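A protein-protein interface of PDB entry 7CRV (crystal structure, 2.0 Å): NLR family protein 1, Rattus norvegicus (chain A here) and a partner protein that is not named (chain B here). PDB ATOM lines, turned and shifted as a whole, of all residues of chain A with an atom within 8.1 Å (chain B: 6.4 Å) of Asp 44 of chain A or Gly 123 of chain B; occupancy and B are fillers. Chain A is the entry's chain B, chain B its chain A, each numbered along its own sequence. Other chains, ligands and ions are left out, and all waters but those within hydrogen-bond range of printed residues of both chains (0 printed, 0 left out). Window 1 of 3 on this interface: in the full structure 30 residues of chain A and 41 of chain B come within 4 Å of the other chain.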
ATOM      1  N   MET A   3       4.025   2.946   9.339  1.00  0.00           N
ATOM      2  CA  MET A   3       4.642   1.929  10.192  1.00  0.00           C
ATOM      3  C   MET A   3       5.743   1.188   9.432  1.00  0.00           C
ATOM      4  O   MET A   3       5.722   1.082   8.199  1.00  0.00           O
ATOM      5  CB  MET A   3       3.583   0.927  10.740  1.00  0.00           C
ATOM      6  CG  MET A   3       2.846   0.149   9.656  1.00  0.00           C
ATOM      7  SD  MET A   3       1.694  -1.117  10.289  1.00  0.00           S
ATOM      8  CE  MET A   3       0.383  -0.075  10.937  1.00  0.00           C
ATOM      9  N   GLY A   4       6.712   0.686  10.185  1.00  0.00           N
ATOM     10  CA  GLY A   4       7.863  -0.006   9.628  1.00  0.00           C
ATOM     11  C   GLY A   4       8.726  -0.445  10.787  1.00  0.00           C
ATOM     12  O   GLY A   4       8.431  -0.142  11.942  1.00  0.00           O
ATOM     13  N   VAL A   5       9.839  -1.112  10.468  1.00  0.00           N
ATOM     14  CA  VAL A   5      10.654  -1.815  11.463  1.00  0.00           C
ATOM     15  C   VAL A   5      11.870  -0.977  11.880  1.00  0.00           C
ATOM     16  O   VAL A   5      12.605  -0.454  11.032  1.00  0.00           O
ATOM     17  CB  VAL A   5      11.084  -3.190  10.931  1.00  0.00           C
ATOM     18  CG1 VAL A   5      11.961  -3.929  11.971  1.00  0.00           C
ATOM     19  CG2 VAL A   5       9.819  -4.025  10.578  1.00  0.00           C
ATOM     20  N   LEU A   6      12.077  -0.862  13.200  1.00  0.00           N
ATOM     21  CA  LEU A   6      13.236  -0.234  13.824  1.00  0.00           C
ATOM     22  C   LEU A   6      14.051  -1.288  14.562  1.00  0.00           C
ATOM     23  O   LEU A   6      13.499  -2.286  15.036  1.00  0.00           O
ATOM     24  CB  LEU A   6      12.810   0.852  14.825  1.00  0.00           C
ATOM     25  CG  LEU A   6      12.196   2.118  14.229  1.00  0.00           C
ATOM     26  CD1 LEU A   6      11.717   3.043  15.347  1.00  0.00           C
ATOM     27  CD2 LEU A   6      13.180   2.850  13.329  1.00  0.00           C
ATOM     28  N   LEU A   7      15.364  -1.070  14.672  1.00  0.00           N
ATOM     29  CA  LEU A   7      16.240  -1.956  15.434  1.00  0.00           C
ATOM     30  C   LEU A   7      16.966  -1.157  16.512  1.00  0.00           C
ATOM     31  O   LEU A   7      17.580  -0.126  16.208  1.00  0.00           O
ATOM     32  CB  LEU A   7      17.255  -2.646  14.527  1.00  0.00           C
ATOM     33  CG  LEU A   7      18.254  -3.574  15.232  1.00  0.00           C
ATOM     34  CD1 LEU A   7      17.552  -4.851  15.757  1.00  0.00           C
ATOM     35  CD2 LEU A   7      19.407  -3.922  14.307  1.00  0.00           C
ATOM     36  N   THR A  20      21.086  -7.094   4.394  1.00  0.00           N
ATOM     37  CA  THR A  20      20.842  -7.498   3.016  1.00  0.00           C
ATOM     38  C   THR A  20      20.928  -6.258   2.134  1.00  0.00           C
ATOM     39  O   THR A  20      20.147  -5.317   2.313  1.00  0.00           O
ATOM     40  CB  THR A  20      19.452  -8.123   2.871  1.00  0.00           C
ATOM     41  OG1 THR A  20      19.267  -9.146   3.852  1.00  0.00           O
ATOM     42  CG2 THR A  20      19.272  -8.720   1.467  1.00  0.00           C
ATOM     43  N   SER A  21      21.855  -6.251   1.186  1.00  0.00           N
ATOM     44  CA  SER A  21      22.008  -5.122   0.280  1.00  0.00           C
ATOM     45  C   SER A  21      21.544  -5.537  -1.103  1.00  0.00           C
ATOM     46  O   SER A  21      21.393  -6.726  -1.393  1.00  0.00           O
ATOM     47  CB  SER A  21      23.460  -4.653   0.227  1.00  0.00           C
ATOM     48  OG  SER A  21      24.228  -5.606  -0.485  1.00  0.00           O
ATOM     49  N   ILE A  22      21.297  -4.548  -1.953  1.00  0.00           N
ATOM     50  CA  ILE A  22      20.952  -4.793  -3.344  1.00  0.00           C
ATOM     51  C   ILE A  22      21.821  -3.891  -4.201  1.00  0.00           C
ATOM     52  O   ILE A  22      22.137  -2.763  -3.814  1.00  0.00           O
ATOM     53  CB  ILE A  22      19.451  -4.559  -3.627  1.00  0.00           C
ATOM     54  CG1 ILE A  22      19.032  -3.169  -3.152  1.00  0.00           C
ATOM     55  CG2 ILE A  22      18.605  -5.647  -2.916  1.00  0.00           C
ATOM     56  CD1 ILE A  22      17.638  -2.758  -3.599  1.00  0.00           C
ATOM     57  N   LEU A  24      21.915  -1.905  -7.739  1.00  0.00           N
ATOM     58  CA  LEU A  24      21.002  -1.401  -8.762  1.00  0.00           C
ATOM     59  C   LEU A  24      21.844  -0.881  -9.912  1.00  0.00           C
ATOM     60  O   LEU A  24      22.693  -0.002  -9.706  1.00  0.00           O
ATOM     61  CB  LEU A  24      20.093  -0.295  -8.203  1.00  0.00           C
ATOM     62  CG  LEU A  24      19.227  -0.711  -7.016  1.00  0.00           C
ATOM     63  CD1 LEU A  24      18.643   0.503  -6.315  1.00  0.00           C
ATOM     64  CD2 LEU A  24      18.128  -1.724  -7.422  1.00  0.00           C
ATOM     65  N   VAL A  41      22.813  -0.355  -2.033  1.00  0.00           N
ATOM     66  CA  VAL A  41      21.918   0.227  -1.036  1.00  0.00           C
ATOM     67  C   VAL A  41      21.279  -0.890  -0.229  1.00  0.00           C
ATOM     68  O   VAL A  41      21.288  -2.062  -0.636  1.00  0.00           O
ATOM     69  CB  VAL A  41      20.823   1.101  -1.685  1.00  0.00           C
ATOM     70  CG1 VAL A  41      21.446   2.308  -2.396  1.00  0.00           C
ATOM     71  CG2 VAL A  41      19.979   0.280  -2.631  1.00  0.00           C
ATOM     72  N   PRO A  42      20.723  -0.556   0.932  1.00  0.00           N
ATOM     73  CA  PRO A  42      19.965  -1.559   1.685  1.00  0.00           C
ATOM     74  C   PRO A  42      18.783  -2.074   0.868  1.00  0.00           C
ATOM     75  O   PRO A  42      18.251  -1.379  -0.004  1.00  0.00           O
ATOM     76  CB  PRO A  42      19.511  -0.788   2.930  1.00  0.00           C
ATOM     77  CG  PRO A  42      20.571   0.286   3.079  1.00  0.00           C
ATOM     78  CD  PRO A  42      20.808   0.722   1.668  1.00  0.00           C
ATOM     79  N   ASN A  43      18.388  -3.321   1.135  1.00  0.00           N
ATOM     80  CA  ASN A  43      17.249  -3.897   0.422  1.00  0.00           C
ATOM     81  C   ASN A  43      15.967  -3.257   0.945  1.00  0.00           C
ATOM     82  O   ASN A  43      15.392  -3.694   1.946  1.00  0.00           O
ATOM     83  CB  ASN A  43      17.217  -5.436   0.569  1.00  0.00           C
ATOM     84  CG  ASN A  43      16.010  -6.058  -0.113  1.00  0.00           C
ATOM     85  OD1 ASN A  43      15.448  -5.470  -1.028  1.00  0.00           O
ATOM     86  ND2 ASN A  43      15.609  -7.250   0.330  1.00  0.00           N
ATOM     87  N   ASP A  44      15.514  -2.206   0.268  1.00  0.00           N
ATOM     88  CA  ASP A  44      14.457  -1.335   0.774  1.00  0.00           C
ATOM     89  C   ASP A  44      13.694  -0.871  -0.455  1.00  0.00           C
ATOM     90  O   ASP A  44      14.221  -0.068  -1.224  1.00  0.00           O
ATOM     91  CB  ASP A  44      15.057  -0.148   1.539  1.00  0.00           C
ATOM     92  CG  ASP A  44      14.004   0.798   2.108  1.00  0.00           C
ATOM     93  OD1 ASP A  44      13.082   1.235   1.364  1.00  0.00           O
ATOM     94  OD2 ASP A  44      14.139   1.173   3.298  1.00  0.00           O
ATOM     95  N   CYS A  45      12.467  -1.351  -0.637  1.00  0.00           N
ATOM     96  CA  CYS A  45      11.730  -1.014  -1.860  1.00  0.00           C
ATOM     97  C   CYS A  45      11.484   0.487  -2.013  1.00  0.00           C
ATOM     98  O   CYS A  45      11.308   0.962  -3.142  1.00  0.00           O
ATOM     99  CB  CYS A  45      10.388  -1.757  -1.897  1.00  0.00           C
ATOM    100  SG  CYS A  45       9.230  -1.247  -0.599  1.00  0.00           S
ATOM    101  N   THR A  46      11.398   1.243  -0.907  1.00  0.00           N
ATOM    102  CA  THR A  46      11.153   2.684  -1.036  1.00  0.00           C
ATOM    103  C   THR A  46      12.397   3.410  -1.542  1.00  0.00           C
ATOM    104  O   THR A  46      12.288   4.435  -2.238  1.00  0.00           O
ATOM    105  CB  THR A  46      10.698   3.285   0.299  1.00  0.00           C
ATOM    106  OG1 THR A  46      11.730   3.141   1.281  1.00  0.00           O
ATOM    107  CG2 THR A  46       9.419   2.583   0.826  1.00  0.00           C
ATOM    108  N   ILE A  47      13.581   2.900  -1.195  1.00  0.00           N
ATOM    109  CA  ILE A  47      14.825   3.439  -1.746  1.00  0.00           C
ATOM    110  C   ILE A  47      14.939   3.104  -3.227  1.00  0.00           C
ATOM    111  O   ILE A  47      15.245   3.971  -4.051  1.00  0.00           O
ATOM    112  CB  ILE A  47      16.035   2.913  -0.954  1.00  0.00           C
ATOM    113  CG1 ILE A  47      16.057   3.531   0.457  1.00  0.00           C
ATOM    114  CG2 ILE A  47      17.351   3.239  -1.660  1.00  0.00           C
ATOM    115  CD1 ILE A  47      17.235   3.063   1.323  1.00  0.00           C
ATOM    116  N   ARG A  48      14.704   1.837  -3.581  1.00  0.00           N
ATOM    117  CA  ARG A  48      14.779   1.439  -4.984  1.00  0.00           C
ATOM    118  C   ARG A  48      13.799   2.242  -5.839  1.00  0.00           C
ATOM    119  O   ARG A  48      14.129   2.637  -6.966  1.00  0.00           O
ATOM    120  CB  ARG A  48      14.511  -0.073  -5.118  1.00  0.00           C
ATOM    121  CG  ARG A  48      14.559  -0.580  -6.559  1.00  0.00           C
ATOM    122  CD  ARG A  48      14.527  -2.088  -6.620  1.00  0.00           C
ATOM    123  NE  ARG A  48      13.150  -2.554  -6.515  1.00  0.00           N
ATOM    124  CZ  ARG A  48      12.726  -3.748  -6.926  1.00  0.00           C
ATOM    125  NH1 ARG A  48      13.564  -4.621  -7.472  1.00  0.00           N
ATOM    126  NH2 ARG A  48      11.454  -4.084  -6.773  1.00  0.00           N
ATOM    127  N   LYS A  49      12.587   2.493  -5.320  1.00  0.00           N
ATOM    128  CA  LYS A  49      11.591   3.294  -6.041  1.00  0.00           C
ATOM    129  C   LYS A  49      12.071   4.721  -6.276  1.00  0.00           C
ATOM    130  O   LYS A  49      11.963   5.241  -7.397  1.00  0.00           O
ATOM    131  CB  LYS A  49      10.250   3.279  -5.293  1.00  0.00           C
ATOM    132  CG  LYS A  49       9.165   4.203  -5.867  1.00  0.00           C
ATOM    133  CD  LYS A  49       8.687   3.890  -7.288  1.00  0.00           C
ATOM    134  CE  LYS A  49       7.736   2.734  -7.436  1.00  0.00           C
ATOM    135  NZ  LYS A  49       7.367   2.632  -8.903  1.00  0.00           N
ATOM    136  N   ALA A  50      12.615   5.376  -5.242  1.00  0.00           N
ATOM    137  CA  ALA A  50      13.058   6.755  -5.439  1.00  0.00           C
ATOM    138  C   ALA A  50      14.232   6.846  -6.404  1.00  0.00           C
ATOM    139  O   ALA A  50      14.342   7.837  -7.138  1.00  0.00           O
ATOM    140  CB  ALA A  50      13.413   7.414  -4.107  1.00  0.00           C
ATOM    141  N   ILE A  51      15.101   5.832  -6.440  1.00  0.00           N
ATOM    142  CA  ILE A  51      16.206   5.851  -7.394  1.00  0.00           C
ATOM    143  C   ILE A  51      15.696   5.628  -8.811  1.00  0.00           C
ATOM    144  O   ILE A  51      16.125   6.319  -9.748  1.00  0.00           O
ATOM    145  CB  ILE A  51      17.293   4.828  -7.006  1.00  0.00           C
ATOM    146  CG1 ILE A  51      17.919   5.196  -5.654  1.00  0.00           C
ATOM    147  CG2 ILE A  51      18.385   4.770  -8.085  1.00  0.00           C
ATOM    148  CD1 ILE A  51      18.792   4.115  -5.064  1.00  0.00           C
ATOM    149  N   TYR A  97      22.557   3.664   4.783  1.00  0.00           N
ATOM    150  CA  TYR A  97      21.156   4.005   4.618  1.00  0.00           C
ATOM    151  C   TYR A  97      21.037   5.511   4.429  1.00  0.00           C
ATOM    152  O   TYR A  97      21.473   6.280   5.292  1.00  0.00           O
ATOM    153  CB  TYR A  97      20.331   3.560   5.823  1.00  0.00           C
ATOM    154  CG  TYR A  97      18.894   3.991   5.677  1.00  0.00           C
ATOM    155  CD1 TYR A  97      18.460   5.217   6.178  1.00  0.00           C
ATOM    156  CD2 TYR A  97      17.984   3.200   4.991  1.00  0.00           C
ATOM    157  CE1 TYR A  97      17.148   5.633   6.026  1.00  0.00           C
ATOM    158  CE2 TYR A  97      16.663   3.603   4.829  1.00  0.00           C
ATOM    159  CZ  TYR A  97      16.256   4.819   5.350  1.00  0.00           C
ATOM    160  OH  TYR A  97      14.956   5.225   5.200  1.00  0.00           O
ATOM    161  N   ARG A  98      20.454   5.926   3.308  1.00  0.00           N
ATOM    162  CA  ARG A  98      20.054   7.308   3.092  1.00  0.00           C
ATOM    163  C   ARG A  98      18.570   7.314   2.762  1.00  0.00           C
ATOM    164  O   ARG A  98      18.084   6.429   2.053  1.00  0.00           O
ATOM    165  CB  ARG A  98      20.878   7.951   1.989  1.00  0.00           C
ATOM    166  CG  ARG A  98      22.332   8.108   2.407  1.00  0.00           C
ATOM    167  CD  ARG A  98      23.240   8.749   1.343  1.00  0.00           C
ATOM    168  NE  ARG A  98      22.586   9.769   0.521  1.00  0.00           N
ATOM    169  CZ  ARG A  98      23.254  10.703  -0.159  1.00  0.00           C
ATOM    170  NH1 ARG A  98      22.598  11.605  -0.885  1.00  0.00           N
ATOM    171  NH2 ARG A  98      24.579  10.721  -0.137  1.00  0.00           N
ATOM    172  N   SER A  99      17.845   8.280   3.332  1.00  0.00           N
ATOM    173  CA  SER A  99      16.397   8.318   3.198  1.00  0.00           C
ATOM    174  C   SER A  99      16.012   8.348   1.715  1.00  0.00           C
ATOM    175  O   SER A  99      16.735   8.925   0.894  1.00  0.00           O
ATOM    176  CB  SER A  99      15.845   9.552   3.925  1.00  0.00           C
ATOM    177  OG  SER A  99      14.463   9.738   3.693  1.00  0.00           O
ATOM    178  N   PRO A 100      14.878   7.711   1.327  1.00  0.00           N
ATOM    179  CA  PRO A 100      14.435   7.841  -0.068  1.00  0.00           C
ATOM    180  C   PRO A 100      14.297   9.291  -0.489  1.00  0.00           C
ATOM    181  O   PRO A 100      14.291   9.569  -1.691  1.00  0.00           O
ATOM    182  CB  PRO A 100      13.081   7.112  -0.097  1.00  0.00           C
ATOM    183  CG  PRO A 100      12.668   6.989   1.321  1.00  0.00           C
ATOM    184  CD  PRO A 100      13.951   6.883   2.113  1.00  0.00           C
ATOM    185  N   ARG A 101      14.194  10.236   0.461  1.00  0.00           N
ATOM    186  CA  ARG A 101      14.045  11.612  -0.002  1.00  0.00           C
ATOM    187  C   ARG A 101      15.382  12.254  -0.348  1.00  0.00           C
ATOM    188  O   ARG A 101      15.393  13.287  -1.017  1.00  0.00           O
ATOM    189  CB  ARG A 101      13.305  12.517   0.999  1.00  0.00           C
ATOM    190  CG  ARG A 101      11.880  12.107   1.479  1.00  0.00           C
ATOM    191  CD  ARG A 101      10.845  11.938   0.328  1.00  0.00           C
ATOM    192  NE  ARG A 101      10.768  10.532  -0.112  1.00  0.00           N
ATOM    193  CZ  ARG A 101       9.923   9.636   0.433  1.00  0.00           C
ATOM    194  NH1 ARG A 101       9.009  10.054   1.319  1.00  0.00           N
ATOM    195  NH2 ARG A 101       9.891   8.357   0.024  1.00  0.00           N
ATOM    196  N   THR B  87       7.745  -5.464  -2.682  1.00  0.00           N
ATOM    197  CA  THR B  87       7.890  -4.651  -1.488  1.00  0.00           C
ATOM    198  C   THR B  87       8.338  -5.443  -0.277  1.00  0.00           C
ATOM    199  O   THR B  87       8.858  -4.845   0.666  1.00  0.00           O
ATOM    200  CB  THR B  87       6.568  -3.948  -1.149  1.00  0.00           C
ATOM    201  OG1 THR B  87       5.559  -4.938  -0.888  1.00  0.00           O
ATOM    202  CG2 THR B  87       6.129  -3.058  -2.311  1.00  0.00           C
ATOM    203  N   TRP B 106      11.272   7.874   6.499  1.00  0.00           N
ATOM    204  CA  TRP B 106      11.349   8.024   7.945  1.00  0.00           C
ATOM    205  C   TRP B 106      11.732   9.441   8.367  1.00  0.00           C
ATOM    206  O   TRP B 106      11.438   9.841   9.500  1.00  0.00           O
ATOM    207  CB  TRP B 106      12.380   7.066   8.505  1.00  0.00           C
ATOM    208  CG  TRP B 106      12.070   5.648   8.366  1.00  0.00           C
ATOM    209  CD1 TRP B 106      12.382   4.838   7.310  1.00  0.00           C
ATOM    210  CD2 TRP B 106      11.456   4.808   9.353  1.00  0.00           C
ATOM    211  NE1 TRP B 106      11.972   3.545   7.571  1.00  0.00           N
ATOM    212  CE2 TRP B 106      11.407   3.503   8.819  1.00  0.00           C
ATOM    213  CE3 TRP B 106      10.949   5.033  10.638  1.00  0.00           C
ATOM    214  CZ2 TRP B 106      10.866   2.422   9.529  1.00  0.00           C
ATOM    215  CZ3 TRP B 106      10.413   3.961  11.341  1.00  0.00           C
ATOM    216  CH2 TRP B 106      10.371   2.662  10.770  1.00  0.00           C
ATOM    217  N   MET B 120      17.517   2.379  15.062  1.00  0.00           N
ATOM    218  CA  MET B 120      17.976   2.502  13.692  1.00  0.00           C
ATOM    219  C   MET B 120      16.863   2.088  12.742  1.00  0.00           C
ATOM    220  O   MET B 120      16.144   1.120  13.015  1.00  0.00           O
ATOM    221  CB  MET B 120      19.155   1.572  13.475  1.00  0.00           C
ATOM    222  CG  MET B 120      20.507   2.131  13.710  1.00  0.00           C
ATOM    223  SD  MET B 120      21.484   0.676  14.009  1.00  0.00           S
ATOM    224  CE  MET B 120      20.981  -0.285  12.575  1.00  0.00           C
ATOM    225  N   VAL B 121      16.780   2.760  11.591  1.00  0.00           N
ATOM    226  CA  VAL B 121      15.903   2.284  10.519  1.00  0.00           C
ATOM    227  C   VAL B 121      16.320   0.879  10.090  1.00  0.00           C
ATOM    228  O   VAL B 121      17.484   0.637   9.746  1.00  0.00           O
ATOM    229  CB  VAL B 121      15.939   3.255   9.325  1.00  0.00           C
ATOM    230  CG1 VAL B 121      15.189   2.626   8.147  1.00  0.00           C
ATOM    231  CG2 VAL B 121      15.291   4.604   9.699  1.00  0.00           C
ATOM    232  N   ALA B 122      15.373  -0.063  10.096  1.00  0.00           N
ATOM    233  CA  ALA B 122      15.688  -1.437   9.718  1.00  0.00           C
ATOM    234  C   ALA B 122      14.856  -1.939   8.543  1.00  0.00           C
ATOM    235  O   ALA B 122      15.036  -3.089   8.119  1.00  0.00           O
ATOM    236  CB  ALA B 122      15.509  -2.378  10.922  1.00  0.00           C
ATOM    237  N   GLY B 123      13.979  -1.103   7.988  1.00  0.00           N
ATOM    238  CA  GLY B 123      13.127  -1.480   6.896  1.00  0.00           C
ATOM    239  C   GLY B 123      12.358  -0.280   6.398  1.00  0.00           C
ATOM    240  O   GLY B 123      12.421   0.816   6.974  1.00  0.00           O
ATOM    241  N   PRO B 124      11.643  -0.458   5.296  1.00  0.00           N
ATOM    242  CA  PRO B 124      10.904   0.655   4.695  1.00  0.00           C
ATOM    243  C   PRO B 124       9.721   1.066   5.549  1.00  0.00           C
ATOM    244  O   PRO B 124       9.187   0.292   6.342  1.00  0.00           O
ATOM    245  CB  PRO B 124      10.430   0.096   3.345  1.00  0.00           C
ATOM    246  CG  PRO B 124      10.491  -1.403   3.494  1.00  0.00           C
ATOM    247  CD  PRO B 124      11.642  -1.666   4.448  1.00  0.00           C
ATOM    248  N   LEU B 125       9.289   2.308   5.350  1.00  0.00           N
ATOM    249  CA  LEU B 125       8.155   2.866   6.068  1.00  0.00           C
ATOM    250  C   LEU B 125       6.957   2.936   5.123  1.00  0.00           C
ATOM    251  O   LEU B 125       7.044   3.547   4.053  1.00  0.00           O
ATOM    252  CB  LEU B 125       8.504   4.248   6.612  1.00  0.00           C
ATOM    253  CG  LEU B 125       7.408   4.850   7.480  1.00  0.00           C
ATOM    254  CD1 LEU B 125       7.292   4.086   8.779  1.00  0.00           C
ATOM    255  CD2 LEU B 125       7.728   6.316   7.760  1.00  0.00           C
ATOM    256  N   PHE B 126       5.856   2.294   5.508  1.00  0.00           N
ATOM    257  CA  PHE B 126       4.624   2.269   4.722  1.00  0.00           C
ATOM    258  C   PHE B 126       3.459   2.890   5.489  1.00  0.00           C
ATOM    259  O   PHE B 126       3.245   2.580   6.667  1.00  0.00           O
ATOM    260  CB  PHE B 126       4.197   0.838   4.359  1.00  0.00           C
ATOM    261  CG  PHE B 126       5.243   0.030   3.636  1.00  0.00           C
ATOM    262  CD1 PHE B 126       5.400   0.139   2.270  1.00  0.00           C
ATOM    263  CD2 PHE B 126       6.025  -0.886   4.325  1.00  0.00           C
ATOM    264  CE1 PHE B 126       6.339  -0.637   1.607  1.00  0.00           C
ATOM    265  CE2 PHE B 126       6.968  -1.648   3.670  1.00  0.00           C
ATOM    266  CZ  PHE B 126       7.120  -1.533   2.317  1.00  0.00           C
ATOM    267  N   PRO B 141       8.612  -5.828   6.006  1.00  0.00           N
ATOM    268  CA  PRO B 141       9.970  -6.251   5.662  1.00  0.00           C
ATOM    269  C   PRO B 141      11.045  -5.483   6.437  1.00  0.00           C
ATOM    270  O   PRO B 141      10.865  -4.335   6.841  1.00  0.00           O
ATOM    271  CB  PRO B 141      10.055  -5.946   4.161  1.00  0.00           C
ATOM    272  CG  PRO B 141       9.102  -4.818   3.978  1.00  0.00           C
ATOM    273  CD  PRO B 141       7.960  -5.120   4.894  1.00  0.00           C
ATOM    274  N   HIS B 142      12.185  -6.134   6.621  1.00  0.00           N
ATOM    275  CA  HIS B 142      13.350  -5.493   7.208  1.00  0.00           C
ATOM    276  C   HIS B 142      14.574  -6.037   6.496  1.00  0.00           C
ATOM    277  O   HIS B 142      14.564  -7.175   6.020  1.00  0.00           O
ATOM    278  CB  HIS B 142      13.424  -5.744   8.725  1.00  0.00           C
ATOM    279  CG  HIS B 142      13.818  -7.146   9.096  1.00  0.00           C
ATOM    280  ND1 HIS B 142      15.094  -7.635   8.916  1.00  0.00           N
ATOM    281  CD2 HIS B 142      13.101  -8.162   9.644  1.00  0.00           C
ATOM    282  CE1 HIS B 142      15.147  -8.889   9.337  1.00  0.00           C
ATOM    283  NE2 HIS B 142      13.954  -9.227   9.792  1.00  0.00           N
ATOM    284  N   PHE B 143      15.635  -5.228   6.418  1.00  0.00           N
ATOM    285  CA  PHE B 143      16.846  -5.663   5.731  1.00  0.00           C
ATOM    286  C   PHE B 143      17.972  -6.086   6.679  1.00  0.00           C
ATOM    287  O   PHE B 143      19.119  -6.209   6.242  1.00  0.00           O
ATOM    288  CB  PHE B 143      17.340  -4.579   4.769  1.00  0.00           C
ATOM    289  CG  PHE B 143      17.348  -3.188   5.352  1.00  0.00           C
ATOM    290  CD1 PHE B 143      18.313  -2.807   6.281  1.00  0.00           C
ATOM    291  CD2 PHE B 143      16.424  -2.253   4.930  1.00  0.00           C
ATOM    292  CE1 PHE B 143      18.318  -1.526   6.786  1.00  0.00           C
ATOM    293  CE2 PHE B 143      16.422  -0.965   5.424  1.00  0.00           C
ATOM    294  CZ  PHE B 143      17.374  -0.596   6.358  1.00  0.00           C
ATOM    295  N   VAL B 144      17.686  -6.334   7.949  1.00  0.00           N
ATOM    296  CA  VAL B 144      18.733  -6.814   8.859  1.00  0.00           C
ATOM    297  C   VAL B 144      19.000  -8.287   8.570  1.00  0.00           C
ATOM    298  O   VAL B 144      18.070  -9.075   8.383  1.00  0.00           O
ATOM    299  CB  VAL B 144      18.326  -6.608  10.333  1.00  0.00           C
ATOM    300  CG1 VAL B 144      19.506  -6.923  11.270  1.00  0.00           C
ATOM    301  CG2 VAL B 144      17.852  -5.190  10.557  1.00  0.00           C
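The backbone carbonyl oxygen of Leu 7 of chain A is in hydrogen-bond range of the backbone NH of Met 120 of chain B. The backbone NH (N) of Thr 20 of chain A is in hydrogen-bond range of the backbone carbonyl oxygen (O) of Phe 143 of chain B, at 2.8 Å. O of Val 5 of chain A is in hydrogen-bond range of N of Gly 123 of chain B (3.4 Å). N of Ala 122 of chain B sits at hydrogen-bond distance from O of Val 5 of chain A, 2.9 Å away. N of Met 3 of chain A lies within hydrogen-bond range of O of Phe 126 of chain B, at 2.8 Å.
The backbone NH (N) of Thr 46 of chain A sits at hydrogen-bond distance from the side-chain carboxylate (OD1) of Asp 44 of chain A (2.8 Å). N of Asn 43 of chain A is in hydrogen-bond range of O of Thr 20 of chain A, 2.9 Å away. The backbone NH (N) of Phe 143 of chain B sits at hydrogen-bond distance from the backbone carbonyl oxygen (O) of Ala 122 of chain B, at 2.8 Å. N of Ile 47 of chain A sits at hydrogen-bond distance from OD1 of Asp 44 of chain A, 3.1 Å away. ND1 of His 142 of chain B lies within hydrogen-bond range of N of Val 144 of chain B (3.1 Å).
Among the printed residues, pairs that only touch across the chains: Leu 6 of chain A with Met 120 of chain B (3.3 Å), Met 3 of chain A with Leu 125 of chain B (3.4 Å), Tyr 97 of chain A with Trp 106 of chain B (3.4 Å), Asn 43 of chain A with Phe 143 of chain B (3.5 Å), Asp 44 of chain A with Pro 124 of chain B (3.5 Å), Gly 4 of chain A with Trp 106 of chain B (3.5 Å), Gly 4 of chain A with Pro 124 of chain B (3.6 Å), Leu 6 of chain A with Trp 106 of chain B (3.6 Å), Cys 45 of chain A with Phe 126 of chain B (3.6 Å), Thr 46 of chain A with Pro 124 of chain B (3.7 Å), Val 5 of chain A with Trp 106 of chain B (3.7 Å), Tyr 97 of chain A with Val 121 of chain B (3.7 Å), Gly 4 of chain A with Leu 125 of chain B (3.7 Å), Cys 45 of chain A with Thr 87 of chain B (3.8 Å), Asp 44 of chain A with Phe 143 of chain B (3.8 Å), Asp 44 of chain A with Gly 123 of chain B (3.9 Å), Val 5 of chain A with Pro 141 of chain B (3.9 Å), Leu 6 of chain A with Val 121 of chain B (3.95 Å), Pro 42 of chain A with Phe 143 of chain B (3.96 Å), Leu 7 of chain A with Ala 122 of chain B (3.97 Å) and Val 5 of chain A with His 142 of chain B (3.996 Å).
Asp 44 of chain A touches just these residues of chain B: Gly 123, Pro 124 and Phe 143. Gly 123 of chain B touches just these residues of chain A: Val 5 (3.4 Å) and Asp 44 (3.9 Å). Of the printed residues of chain A, Phe 126 of chain B touches Met 3 (2.8 Å) and Cys 45 (3.6 Å). Of the printed residues of chain B, Leu 7 of chain A touches Met 120 (2.8 Å) and Ala 122 (3.97 Å). Ser 99 of chain A touches none of the printed residues of chain B. Arg 98 of chain A touches none of the printed residues of chain B. The nearest residue of chain B that does not touch Asp 44 of chain A is Val 121 of chain B (5.2 Å). The nearest printed residue of chain A that does not touch Thr 87 of chain B is Arg 48 of chain A (5.7 Å).
Of the 25 printed residues of chain A, 12 touch a printed residue of chain B. Hydrophobic or aromatic side chains of chain A that line the printed part of chain B: Met 3, Val 5, Leu 6, Pro 42 and Tyr 97. Printed residues of chain B that touch a printed residue of chain A: Thr 87, Trp 106, Met 120, Val 121, Ala 122, Gly 123, Pro 124, Leu 125, Phe 126, Pro 141, His 142 and Phe 143. Hydrophobic or aromatic side chains of chain B that line the printed part of chain A: Trp 106, Met 120, Val 121, Ala 122, Pro 124, Leu 125, Phe 126, His 142 and Phe 143. Along chain B the printed residues that touch a printed residue of chain A span positions 87 to 143.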
